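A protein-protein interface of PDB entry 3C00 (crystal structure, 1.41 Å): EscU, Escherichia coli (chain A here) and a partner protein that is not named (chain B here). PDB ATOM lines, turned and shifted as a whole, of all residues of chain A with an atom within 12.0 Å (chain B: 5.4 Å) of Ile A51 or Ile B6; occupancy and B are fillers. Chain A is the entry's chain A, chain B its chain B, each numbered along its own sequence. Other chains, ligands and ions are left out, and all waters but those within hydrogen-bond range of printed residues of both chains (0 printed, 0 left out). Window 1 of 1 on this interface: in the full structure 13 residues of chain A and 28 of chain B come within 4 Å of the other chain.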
ATOM      1  N   LEU A  41      20.459 -32.010  13.199  1.00  0.00           N
ATOM      2  CA  LEU A  41      21.352 -30.848  13.439  1.00  0.00           C
ATOM      3  C   LEU A  41      20.830 -30.018  14.628  1.00  0.00           C
ATOM      4  O   LEU A  41      21.579 -29.623  15.520  1.00  0.00           O
ATOM      5  CB  LEU A  41      21.400 -29.993  12.169  1.00  0.00           C
ATOM      6  CG  LEU A  41      22.196 -28.694  12.134  1.00  0.00           C
ATOM      7  CD1 LEU A  41      23.644 -28.970  12.455  1.00  0.00           C
ATOM      8  CD2 LEU A  41      22.047 -27.993  10.771  1.00  0.00           C
ATOM      9  N   ALA A  42      19.533 -29.757  14.635  1.00  0.00           N
ATOM     10  CA  ALA A  42      18.900 -29.002  15.717  1.00  0.00           C
ATOM     11  C   ALA A  42      19.182 -29.670  17.040  1.00  0.00           C
ATOM     12  O   ALA A  42      19.536 -29.004  18.020  1.00  0.00           O
ATOM     13  CB  ALA A  42      17.420 -28.914  15.491  1.00  0.00           C
ATOM     14  N   ASN A  43      18.979 -30.987  17.072  1.00  0.00           N
ATOM     15  CA  ASN A  43      19.066 -31.773  18.319  1.00  0.00           C
ATOM     16  C   ASN A  43      20.465 -31.810  18.840  1.00  0.00           C
ATOM     17  O   ASN A  43      20.716 -31.844  20.056  1.00  0.00           O
ATOM     18  CB  ASN A  43      18.566 -33.207  18.106  1.00  0.00           C
ATOM     19  CG  ASN A  43      17.086 -33.334  18.300  1.00  0.00           C
ATOM     20  OD1 ASN A  43      16.437 -32.445  18.854  1.00  0.00           O
ATOM     21  ND2 ASN A  43      16.529 -34.456  17.858  1.00  0.00           N
ATOM     22  N   ASN A  44      21.406 -31.810  17.913  1.00  0.00           N
ATOM     23  CA  ASN A  44      22.776 -31.603  18.278  1.00  0.00           C
ATOM     24  C   ASN A  44      23.074 -30.172  18.754  1.00  0.00           C
ATOM     25  O   ASN A  44      23.531 -29.959  19.892  1.00  0.00           O
ATOM     26  CB  ASN A  44      23.670 -31.929  17.101  1.00  0.00           C
ATOM     27  CG  ASN A  44      25.080 -32.055  17.519  1.00  0.00           C
ATOM     28  OD1 ASN A  44      25.351 -32.260  18.706  1.00  0.00           O
ATOM     29  ND2 ASN A  44      26.002 -31.942  16.577  1.00  0.00           N
ATOM     30  N   ILE A  45      22.877 -29.232  17.838  1.00  0.00           N
ATOM     31  CA  ILE A  45      23.154 -27.810  18.019  1.00  0.00           C
ATOM     32  C   ILE A  45      22.641 -27.159  19.306  1.00  0.00           C
ATOM     33  O   ILE A  45      23.291 -26.283  19.858  1.00  0.00           O
ATOM     34  CB  ILE A  45      22.628 -27.000  16.749  1.00  0.00           C
ATOM     35  CG1 ILE A  45      23.759 -26.752  15.748  1.00  0.00           C
ATOM     36  CG2 ILE A  45      21.983 -25.672  17.125  1.00  0.00           C
ATOM     37  CD1 ILE A  45      23.373 -25.771  14.736  1.00  0.00           C
ATOM     38  N   LYS A  46      21.442 -27.551  19.727  1.00  0.00           N
ATOM     39  CA  LYS A  46      20.689 -26.754  20.713  1.00  0.00           C
ATOM     40  C   LYS A  46      21.391 -26.593  22.069  1.00  0.00           C
ATOM     41  O   LYS A  46      21.104 -25.659  22.797  1.00  0.00           O
ATOM     42  CB  LYS A  46      19.267 -27.323  20.915  1.00  0.00           C
ATOM     43  CG  LYS A  46      19.238 -28.692  21.573  1.00  0.00           C
ATOM     44  CD  LYS A  46      17.897 -29.406  21.393  1.00  0.00           C
ATOM     45  CE  LYS A  46      18.021 -30.863  21.783  1.00  0.00           C
ATOM     46  NZ  LYS A  46      16.910 -31.675  21.220  1.00  0.00           N
ATOM     47  N   LYS A  47      22.297 -27.498  22.412  1.00  0.00           N
ATOM     48  CA  LYS A  47      23.051 -27.383  23.658  1.00  0.00           C
ATOM     49  C   LYS A  47      24.242 -26.441  23.552  1.00  0.00           C
ATOM     50  O   LYS A  47      24.932 -26.270  24.520  1.00  0.00           O
ATOM     51  CB  LYS A  47      23.542 -28.766  24.125  1.00  0.00           C
ATOM     52  CG  LYS A  47      24.630 -29.419  23.247  1.00  0.00           C
ATOM     53  CD  LYS A  47      24.923 -30.834  23.739  1.00  0.00           C
ATOM     54  CE  LYS A  47      26.098 -31.472  23.032  1.00  0.00           C
ATOM     55  NZ  LYS A  47      26.367 -32.786  23.617  1.00  0.00           N
ATOM     56  N   SER A  48      24.502 -25.857  22.395  1.00  0.00           N
ATOM     57  CA  SER A  48      25.728 -25.096  22.186  1.00  0.00           C
ATOM     58  C   SER A  48      25.862 -23.939  23.154  1.00  0.00           C
ATOM     59  O   SER A  48      24.880 -23.300  23.480  1.00  0.00           O
ATOM     60  CB  SER A  48      25.776 -24.517  20.764  1.00  0.00           C
ATOM     61  OG  SER A  48      25.895 -25.504  19.768  1.00  0.00           O
ATOM     62  N   THR A  49      27.100 -23.639  23.547  1.00  0.00           N
ATOM     63  CA  THR A  49      27.368 -22.517  24.424  1.00  0.00           C
ATOM     64  C   THR A  49      27.488 -21.221  23.616  1.00  0.00           C
ATOM     65  O   THR A  49      27.005 -20.183  24.032  1.00  0.00           O
ATOM     66  CB  THR A  49      28.672 -22.827  25.173  1.00  0.00           C
ATOM     67  OG1 THR A  49      28.573 -24.114  25.816  1.00  0.00           O
ATOM     68  CG2 THR A  49      28.994 -21.719  26.212  1.00  0.00           C
ATOM     69  N   VAL A  50      28.124 -21.295  22.453  1.00  0.00           N
ATOM     70  CA  VAL A  50      28.351 -20.129  21.628  1.00  0.00           C
ATOM     71  C   VAL A  50      28.651 -20.641  20.226  1.00  0.00           C
ATOM     72  O   VAL A  50      29.231 -21.724  20.061  1.00  0.00           O
ATOM     73  CB  VAL A  50      29.488 -19.238  22.160  1.00  0.00           C
ATOM     74  CG1 VAL A  50      30.804 -19.995  22.163  1.00  0.00           C
ATOM     75  CG2 VAL A  50      29.595 -17.917  21.353  1.00  0.00           C
ATOM     76  N   ILE A  51      28.211 -19.882  19.228  1.00  0.00           N
ATOM     77  CA  ILE A  51      28.479 -20.139  17.818  1.00  0.00           C
ATOM     78  C   ILE A  51      29.297 -18.999  17.274  1.00  0.00           C
ATOM     79  O   ILE A  51      28.992 -17.852  17.532  1.00  0.00           O
ATOM     80  CB  ILE A  51      27.176 -20.317  17.054  1.00  0.00           C
ATOM     81  CG1 ILE A  51      26.522 -21.613  17.542  1.00  0.00           C
ATOM     82  CG2 ILE A  51      27.414 -20.328  15.516  1.00  0.00           C
ATOM     83  CD1 ILE A  51      25.081 -21.796  17.156  1.00  0.00           C
ATOM     84  N   VAL A  52      30.377 -19.338  16.588  1.00  0.00           N
ATOM     85  CA  VAL A  52      31.242 -18.363  15.957  1.00  0.00           C
ATOM     86  C   VAL A  52      31.038 -18.469  14.449  1.00  0.00           C
ATOM     87  O   VAL A  52      31.060 -19.566  13.886  1.00  0.00           O
ATOM     88  CB  VAL A  52      32.734 -18.585  16.315  1.00  0.00           C
ATOM     89  CG1 VAL A  52      33.612 -17.435  15.821  1.00  0.00           C
ATOM     90  CG2 VAL A  52      32.887 -18.764  17.785  1.00  0.00           C
ATOM     91  N   LYS A  53      30.857 -17.313  13.812  1.00  0.00           N
ATOM     92  CA  LYS A  53      30.683 -17.277  12.374  1.00  0.00           C
ATOM     93  C   LYS A  53      31.673 -16.299  11.733  1.00  0.00           C
ATOM     94  O   LYS A  53      32.240 -15.428  12.399  1.00  0.00           O
ATOM     95  CB  LYS A  53      29.237 -16.891  11.993  1.00  0.00           C
ATOM     96  CG  LYS A  53      28.813 -15.540  12.512  1.00  0.00           C
ATOM     97  CD  LYS A  53      27.408 -15.130  12.029  1.00  0.00           C
ATOM     98  CE  LYS A  53      27.042 -13.726  12.455  1.00  0.00           C
ATOM     99  NZ  LYS A  53      25.724 -13.287  11.881  1.00  0.00           N
ATOM    100  N   ASN A  54      31.883 -16.455  10.427  1.00  0.00           N
ATOM    101  CA  ASN A  54      32.592 -15.450   9.640  1.00  0.00           C
ATOM    102  C   ASN A  54      31.599 -14.437   9.077  1.00  0.00           C
ATOM    103  O   ASN A  54      31.870 -13.762   8.084  1.00  0.00           O
ATOM    104  CB  ASN A  54      33.443 -16.095   8.544  1.00  0.00           C
ATOM    105  CG  ASN A  54      32.626 -16.678   7.403  1.00  0.00           C
ATOM    106  OD1 ASN A  54      31.413 -16.940   7.535  1.00  0.00           O
ATOM    107  ND2 ASN A  54      33.295 -16.928   6.291  1.00  0.00           N
ATOM    108  OXT ASN A  54      30.478 -14.313   9.599  1.00  0.00           O
ATOM    109  N   ILE B   4      30.883 -19.707   7.118  1.00  0.00           N
ATOM    110  CA  ILE B   4      31.344 -20.668   8.139  1.00  0.00           C
ATOM    111  C   ILE B   4      30.595 -20.458   9.431  1.00  0.00           C
ATOM    112  O   ILE B   4      30.369 -19.337   9.848  1.00  0.00           O
ATOM    113  CB  ILE B   4      32.842 -20.437   8.430  1.00  0.00           C
ATOM    114  CG1 ILE B   4      33.683 -20.732   7.205  1.00  0.00           C
ATOM    115  CG2 ILE B   4      33.293 -21.255   9.633  1.00  0.00           C
ATOM    116  CD1 ILE B   4      35.131 -20.398   7.404  1.00  0.00           C
ATOM    117  N   ALA B   5      30.249 -21.563  10.094  1.00  0.00           N
ATOM    118  CA  ALA B   5      29.746 -21.516  11.462  1.00  0.00           C
ATOM    119  C   ALA B   5      30.341 -22.650  12.262  1.00  0.00           C
ATOM    120  O   ALA B   5      30.420 -23.787  11.791  1.00  0.00           O
ATOM    121  CB  ALA B   5      28.229 -21.641  11.488  1.00  0.00           C
ATOM    122  N   ILE B   6      30.747 -22.335  13.497  1.00  0.00           N
ATOM    123  CA  ILE B   6      31.409 -23.301  14.418  1.00  0.00           C
ATOM    124  C   ILE B   6      30.625 -23.282  15.723  1.00  0.00           C
ATOM    125  O   ILE B   6      30.438 -22.231  16.320  1.00  0.00           O
ATOM    126  CB  ILE B   6      32.850 -22.901  14.729  1.00  0.00           C
ATOM    127  CG1 ILE B   6      33.679 -22.668  13.464  1.00  0.00           C
ATOM    128  CG2 ILE B   6      33.516 -23.976  15.560  1.00  0.00           C
ATOM    129  CD1 ILE B   6      33.833 -23.845  12.553  1.00  0.00           C
ATOM    130  N   CYS B   7      30.123 -24.441  16.112  1.00  0.00           N
ATOM    131  CA  CYS B   7      29.364 -24.594  17.341  1.00  0.00           C
ATOM    132  C   CYS B   7      30.267 -25.128  18.447  1.00  0.00           C
ATOM    133  O   CYS B   7      30.791 -26.226  18.339  1.00  0.00           O
ATOM    134  CB  CYS B   7      28.230 -25.576  17.151  1.00  0.00           C
ATOM    135  SG  CYS B   7      27.061 -25.070  15.874  1.00  0.00           S
ATOM    136  N   LEU B   8      30.405 -24.340  19.496  1.00  0.00           N
ATOM    137  CA  LEU B   8      31.273 -24.637  20.644  1.00  0.00           C
ATOM    138  C   LEU B   8      30.428 -24.976  21.867  1.00  0.00           C
ATOM    139  O   LEU B   8      29.412 -24.332  22.131  1.00  0.00           O
ATOM    140  CB  LEU B   8      32.183 -23.441  20.957  1.00  0.00           C
ATOM    141  CG  LEU B   8      33.328 -23.245  19.959  1.00  0.00           C
ATOM    142  CD1 LEU B   8      33.819 -21.785  20.004  1.00  0.00           C
ATOM    143  CD2 LEU B   8      34.532 -24.183  20.246  1.00  0.00           C
ATOM    144  N   VAL B  20      34.280 -28.509  19.874  1.00  0.00           N
ATOM    145  CA  VAL B  20      33.522 -28.220  18.647  1.00  0.00           C
ATOM    146  C   VAL B  20      32.562 -29.345  18.411  1.00  0.00           C
ATOM    147  O   VAL B  20      32.966 -30.459  18.165  1.00  0.00           O
ATOM    148  CB  VAL B  20      34.463 -28.029  17.463  1.00  0.00           C
ATOM    149  CG1 VAL B  20      33.700 -27.908  16.180  1.00  0.00           C
ATOM    150  CG2 VAL B  20      35.292 -26.745  17.647  1.00  0.00           C
ATOM    151  N   GLU B  22      29.814 -29.150  16.259  1.00  0.00           N
ATOM    152  CA  GLU B  22      29.245 -29.088  14.921  1.00  0.00           C
ATOM    153  C   GLU B  22      29.896 -27.976  14.170  1.00  0.00           C
ATOM    154  O   GLU B  22      30.277 -26.975  14.744  1.00  0.00           O
ATOM    155  CB  GLU B  22      27.726 -28.835  15.010  1.00  0.00           C
ATOM    156  CG  GLU B  22      26.972 -28.973  13.696  1.00  0.00           C
ATOM    157  CD  GLU B  22      26.954 -30.364  13.251  1.00  0.00           C
ATOM    158  OE1 GLU B  22      26.187 -31.179  13.842  1.00  0.00           O
ATOM    159  OE2 GLU B  22      27.729 -30.661  12.343  1.00  0.00           O
ATOM    160  N   THR B  23      30.018 -28.168  12.869  1.00  0.00           N
ATOM    161  CA  THR B  23      30.487 -27.148  11.984  1.00  0.00           C
ATOM    162  C   THR B  23      29.633 -27.124  10.738  1.00  0.00           C
ATOM    163  O   THR B  23      28.933 -28.072  10.398  1.00  0.00           O
ATOM    164  CB  THR B  23      31.932 -27.369  11.565  1.00  0.00           C
ATOM    165  OG1 THR B  23      32.017 -28.529  10.735  1.00  0.00           O
ATOM    166  CG2 THR B  23      32.831 -27.541  12.771  1.00  0.00           C
ATOM    167  N   GLY B  24      29.706 -26.026  10.011  1.00  0.00           N
ATOM    168  CA  GLY B  24      29.052 -26.007   8.698  1.00  0.00           C
ATOM    169  C   GLY B  24      29.700 -24.981   7.817  1.00  0.00           C
ATOM    170  O   GLY B  24      30.200 -23.962   8.301  1.00  0.00           O
ATOM    171  N   ILE B  32      22.685 -23.348  10.485  1.00  0.00           N
ATOM    172  CA  ILE B  32      23.111 -23.292  11.870  1.00  0.00           C
ATOM    173  C   ILE B  32      22.794 -21.940  12.478  1.00  0.00           C
ATOM    174  O   ILE B  32      22.331 -21.860  13.601  1.00  0.00           O
ATOM    175  CB  ILE B  32      24.639 -23.610  12.021  1.00  0.00           C
ATOM    176  CG1 ILE B  32      24.929 -25.083  11.747  1.00  0.00           C
ATOM    177  CG2 ILE B  32      25.199 -23.136  13.377  1.00  0.00           C
ATOM    178  CD1 ILE B  32      26.405 -25.401  11.564  1.00  0.00           C
ATOM    179  N   ILE B  33      23.058 -20.876  11.750  1.00  0.00           N
ATOM    180  CA  ILE B  33      22.787 -19.529  12.242  1.00  0.00           C
ATOM    181  C   ILE B  33      21.287 -19.291  12.443  1.00  0.00           C
ATOM    182  O   ILE B  33      20.892 -18.695  13.437  1.00  0.00           O
ATOM    183  CB  ILE B  33      23.477 -18.478  11.351  1.00  0.00           C
ATOM    184  CG1 ILE B  33      25.008 -18.682  11.384  1.00  0.00           C
ATOM    185  CG2 ILE B  33      23.117 -17.043  11.748  1.00  0.00           C
ATOM    186  CD1 ILE B  33      25.794 -18.018  10.221  1.00  0.00           C
ATOM    187  N   ALA B  36      20.346 -21.148  15.489  1.00  0.00           N
ATOM    188  CA  ALA B  36      20.789 -20.412  16.670  1.00  0.00           C
ATOM    189  C   ALA B  36      19.808 -19.325  17.095  1.00  0.00           C
ATOM    190  O   ALA B  36      19.560 -19.146  18.280  1.00  0.00           O
ATOM    191  CB  ALA B  36      22.177 -19.811  16.452  1.00  0.00           C
ATOM    192  N   ILE B  41      20.765 -19.081  20.928  1.00  0.00           N
ATOM    193  CA  ILE B  41      22.154 -19.401  21.222  1.00  0.00           C
ATOM    194  C   ILE B  41      22.994 -18.218  20.797  1.00  0.00           C
ATOM    195  O   ILE B  41      22.821 -17.723  19.699  1.00  0.00           O
ATOM    196  CB  ILE B  41      22.627 -20.640  20.403  1.00  0.00           C
ATOM    197  CG1 ILE B  41      21.736 -21.874  20.694  1.00  0.00           C
ATOM    198  CG2 ILE B  41      24.110 -20.913  20.645  1.00  0.00           C
ATOM    199  CD1 ILE B  41      21.900 -23.036  19.717  1.00  0.00           C
ATOM    200  N   PRO B  42      23.927 -17.731  21.653  1.00  0.00           N
ATOM    201  CA  PRO B  42      24.786 -16.626  21.282  1.00  0.00           C
ATOM    202  C   PRO B  42      25.575 -16.878  20.012  1.00  0.00           C
ATOM    203  O   PRO B  42      26.194 -17.931  19.876  1.00  0.00           O
ATOM    204  CB  PRO B  42      25.743 -16.534  22.488  1.00  0.00           C
ATOM    205  CG  PRO B  42      24.987 -17.008  23.585  1.00  0.00           C
ATOM    206  CD  PRO B  42      24.195 -18.147  23.043  1.00  0.00           C
ATOM    207  N   VAL B  43      25.531 -15.950  19.073  1.00  0.00           N
ATOM    208  CA  VAL B  43      26.275 -15.983  17.836  1.00  0.00           C
ATOM    209  C   VAL B  43      27.207 -14.784  17.770  1.00  0.00           C
ATOM    210  O   VAL B  43      26.756 -13.616  17.878  1.00  0.00           O
ATOM    211  CB  VAL B  43      25.341 -15.984  16.610  1.00  0.00           C
ATOM    212  CG1 VAL B  43      26.130 -15.902  15.293  1.00  0.00           C
ATOM    213  CG2 VAL B  43      24.491 -17.214  16.632  1.00  0.00           C
ATOM    214  N   ILE B  44      28.489 -15.053  17.547  1.00  0.00           N
ATOM    215  CA  ILE B  44      29.492 -13.984  17.495  1.00  0.00           C
ATOM    216  C   ILE B  44      30.251 -14.051  16.169  1.00  0.00           C
ATOM    217  O   ILE B  44      30.673 -15.133  15.762  1.00  0.00           O
ATOM    218  CB  ILE B  44      30.429 -14.091  18.728  1.00  0.00           C
ATOM    219  CG1 ILE B  44      29.620 -13.934  20.035  1.00  0.00           C
ATOM    220  CG2 ILE B  44      31.555 -13.053  18.627  1.00  0.00           C
ATOM    221  CD1 ILE B  44      30.402 -14.146  21.328  1.00  0.00           C
ATOM    222  N   ALA B  50      36.829 -17.816  13.076  1.00  0.00           N
ATOM    223  CA  ALA B  50      35.963 -18.778  12.409  1.00  0.00           C
ATOM    224  C   ALA B  50      36.761 -19.598  11.388  1.00  0.00           C
ATOM    225  O   ALA B  50      36.654 -20.827  11.365  1.00  0.00           O
ATOM    226  CB  ALA B  50      34.755 -18.099  11.734  1.00  0.00           C
ATOM    227  N   LEU B  53      39.339 -21.947  13.192  1.00  0.00           N
ATOM    228  CA  LEU B  53      38.682 -23.060  13.831  1.00  0.00           C
ATOM    229  C   LEU B  53      38.205 -24.050  12.766  1.00  0.00           C
ATOM    230  O   LEU B  53      38.337 -25.269  12.910  1.00  0.00           O
ATOM    231  CB  LEU B  53      37.491 -22.590  14.695  1.00  0.00           C
ATOM    232  CG  LEU B  53      37.810 -21.939  16.024  1.00  0.00           C
ATOM    233  CD1 LEU B  53      36.586 -21.151  16.560  1.00  0.00           C
ATOM    234  CD2 LEU B  53      38.318 -22.949  17.030  1.00  0.00           C
ATOM    235  N   TYR B  54      37.630 -23.537  11.683  1.00  0.00           N
ATOM    236  CA  TYR B  54      37.112 -24.437  10.677  1.00  0.00           C
ATOM    237  C   TYR B  54      38.205 -25.330  10.069  1.00  0.00           C
ATOM    238  O   TYR B  54      38.030 -26.523   9.850  1.00  0.00           O
ATOM    239  CB  TYR B  54      36.451 -23.644   9.552  1.00  0.00           C
ATOM    240  CG  TYR B  54      35.722 -24.524   8.574  1.00  0.00           C
ATOM    241  CD1 TYR B  54      36.363 -25.010   7.457  1.00  0.00           C
ATOM    242  CD2 TYR B  54      34.405 -24.907   8.785  1.00  0.00           C
ATOM    243  CE1 TYR B  54      35.708 -25.829   6.566  1.00  0.00           C
ATOM    244  CE2 TYR B  54      33.750 -25.722   7.883  1.00  0.00           C
ATOM    245  CZ  TYR B  54      34.412 -26.167   6.779  1.00  0.00           C
ATOM    246  OH  TYR B  54      33.793 -27.003   5.868  1.00  0.00           O
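ND2 of Asn A44 sits at hydrogen-bond distance from OE1 of Glu B22 (2.8 Å).
The backbone NH of Thr A49 is in hydrogen-bond range of the backbone carbonyl oxygen of Leu B8, 2.8 Å away.
O of Val A50 lies within hydrogen-bond range of N of Leu B8, at 2.9 Å.
The backbone NH (N) of Ile A51 lies within hydrogen-bond range of the backbone carbonyl oxygen (O) of Pro B42 (2.9 Å).
The backbone carbonyl oxygen of Ile A51 is in hydrogen-bond range of the backbone NH of Ile B44 (2.8 Å).
O of Val A52 is in hydrogen-bond range of N of Ile B6 (2.8 Å).
The backbone NH of Lys A53 is in hydrogen-bond range of the backbone carbonyl oxygen of Ile B44 (2.9 Å).
The side-chain amide oxygen (OD1) of Asn A54 sits at hydrogen-bond distance from the backbone NH (N) of Ile B4 (2.8 Å).
The backbone carbonyl oxygen of Ile A45 sits at hydrogen-bond distance from the side-chain hydroxyl of Ser A48.
The backbone carbonyl oxygen (O) of Ala B5 is in hydrogen-bond range of the backbone NH (N) of Gly B24 (2.9 Å).
N of Cys B7 is in hydrogen-bond range of O of Glu B22 (2.9 Å).
O of Ala B36 lies within hydrogen-bond range of N of Ile B41 (2.9 Å).
Among the printed residues, merely in contact across the chains: Ile A51 with Ile B6 (3.2 Å), Lys A53 with Ile B4 (3.3 Å), Val A52 with Ile B44 (3.3 Å), Ile A51 with Val B43 (3.3 Å), Val A52 with Ala B5 (3.4 Å), Ile A45 with Ile B32 (3.4 Å), Ser A48 with Cys B7 (3.5 Å), Ile A45 with Ile B41 (3.5 Å), Val A50 with Pro B42 (3.5 Å), Leu A41 with Glu B22 (3.6 Å), Asn A54 with Ala B50 (3.6 Å), Lys A53 with Ala B50 (3.6 Å), Ile A51 with Ala B36 (3.6 Å), Lys A53 with Val B43 (3.6 Å), Thr A49 with Pro B42 (3.6 Å), Ile A45 with Cys B7 (3.7 Å), Ser A48 with Leu B8 (3.7 Å), Ile A51 with Ile B41 (3.7 Å), Lys A53 with Ile B33 (3.8 Å), Ser A48 with Ile B41 (3.8 Å), Val A50 with Ile B44 (3.9 Å), Val A52 with Leu B8 (3.9 Å), Ile A51 with Cys B7 (3.9 Å), Val A50 with Cys B7 (3.9 Å) and Val A50 with Ile B6 (3.96 Å).
Of the printed residues of chain B, Leu A41 touches Glu B22.
Ala A42 touches none of the printed residues of chain B.
Asn A43 touches none of the printed residues of chain B.
Of the printed residues of chain B, Asn A44 touches Glu B22.
Printed residues of chain B within 4 Å of Ile A45: Cys B7 (3.7 Å), Ile B32 (3.4 Å) and Ile B41 (3.5 Å).
Printed residues of chain B within 4 Å of Ile A51: Ile B6 (3.2 Å), Cys B7 (3.9 Å), Ala B36 (3.6 Å), Ile B41 (3.7 Å), Pro B42 (2.9 Å), Val B43 (3.3 Å) and Ile B44 (2.8 Å).
Ile B4 touches just these residues of chain A: Lys A53 (3.3 Å) and Asn A54 (2.8 Å).
Of the printed residues of chain A, Ala B5 touches Val A52 (3.4 Å).
Of chain A, only Val A50 (3.96 Å), Ile A51 (3.2 Å) and Val A52 (2.8 Å) come within 4 Å of Ile B6.
Printed residues of chain A within 4 Å of Leu B8: Ser A48 (3.7 Å), Thr A49 (2.8 Å), Val A50 (2.9 Å) and Val A52 (3.9 Å).
No residue of chain A comes within 4 Å of Gly B24.
Printed residues of chain A within 4 Å of Ile B32: Ile A45 (3.4 Å).
Of chain A, only Lys A53 comes within 4 Å of Ile B33.
Of the printed residues of chain A, Ala B36 touches Ile A51 (3.6 Å).
Pro B42 touches just these residues of chain A: Thr A49 (3.6 Å), Val A50 (3.5 Å) and Ile A51 (2.9 Å).
Of the printed residues of chain A, Val B43 touches Ile A51 (3.3 Å) and Lys A53 (3.6 Å).
Ile B44 touches just these residues of chain A: Val A50 (3.9 Å), Ile A51 (2.8 Å), Val A52 (3.3 Å) and Lys A53 (2.9 Å).
Of chain A, only Lys A53 (3.6 Å) and Asn A54 (3.6 Å) come within 4 Å of Ala B50.
No residue of chain A comes within 4 Å of Leu B53.
The nearest printed residue of chain B that does not touch Ile A51 is Ile B32 (4.01 Å).
The nearest residue of chain A that does not touch Ile B6 is Lys A53 (5.0 Å).
Of the 19 printed residues of chain B, 14 touch a printed residue of chain A.
Printed residues of chain B that touch a printed residue of chain A: Ile B4, Ala B5, Ile B6, Cys B7, Leu B8, Glu B22, Ile B32, Ile B33, Ala B36, Ile B41, Pro B42, Val B43, Ile B44 and Ala B50.
Hydrophobic or aromatic side chains of chain A within 4 Å of the printed part of chain B: Leu A41, Ile A45, Val A50, Ile A51 and Val A52.
Among the printed residues, 33 pairs touch across the chains.
Among the printed residues, no Asp or Glu carboxylate lies within 4 Å of a Lys or Arg side-chain nitrogen of the other chain.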
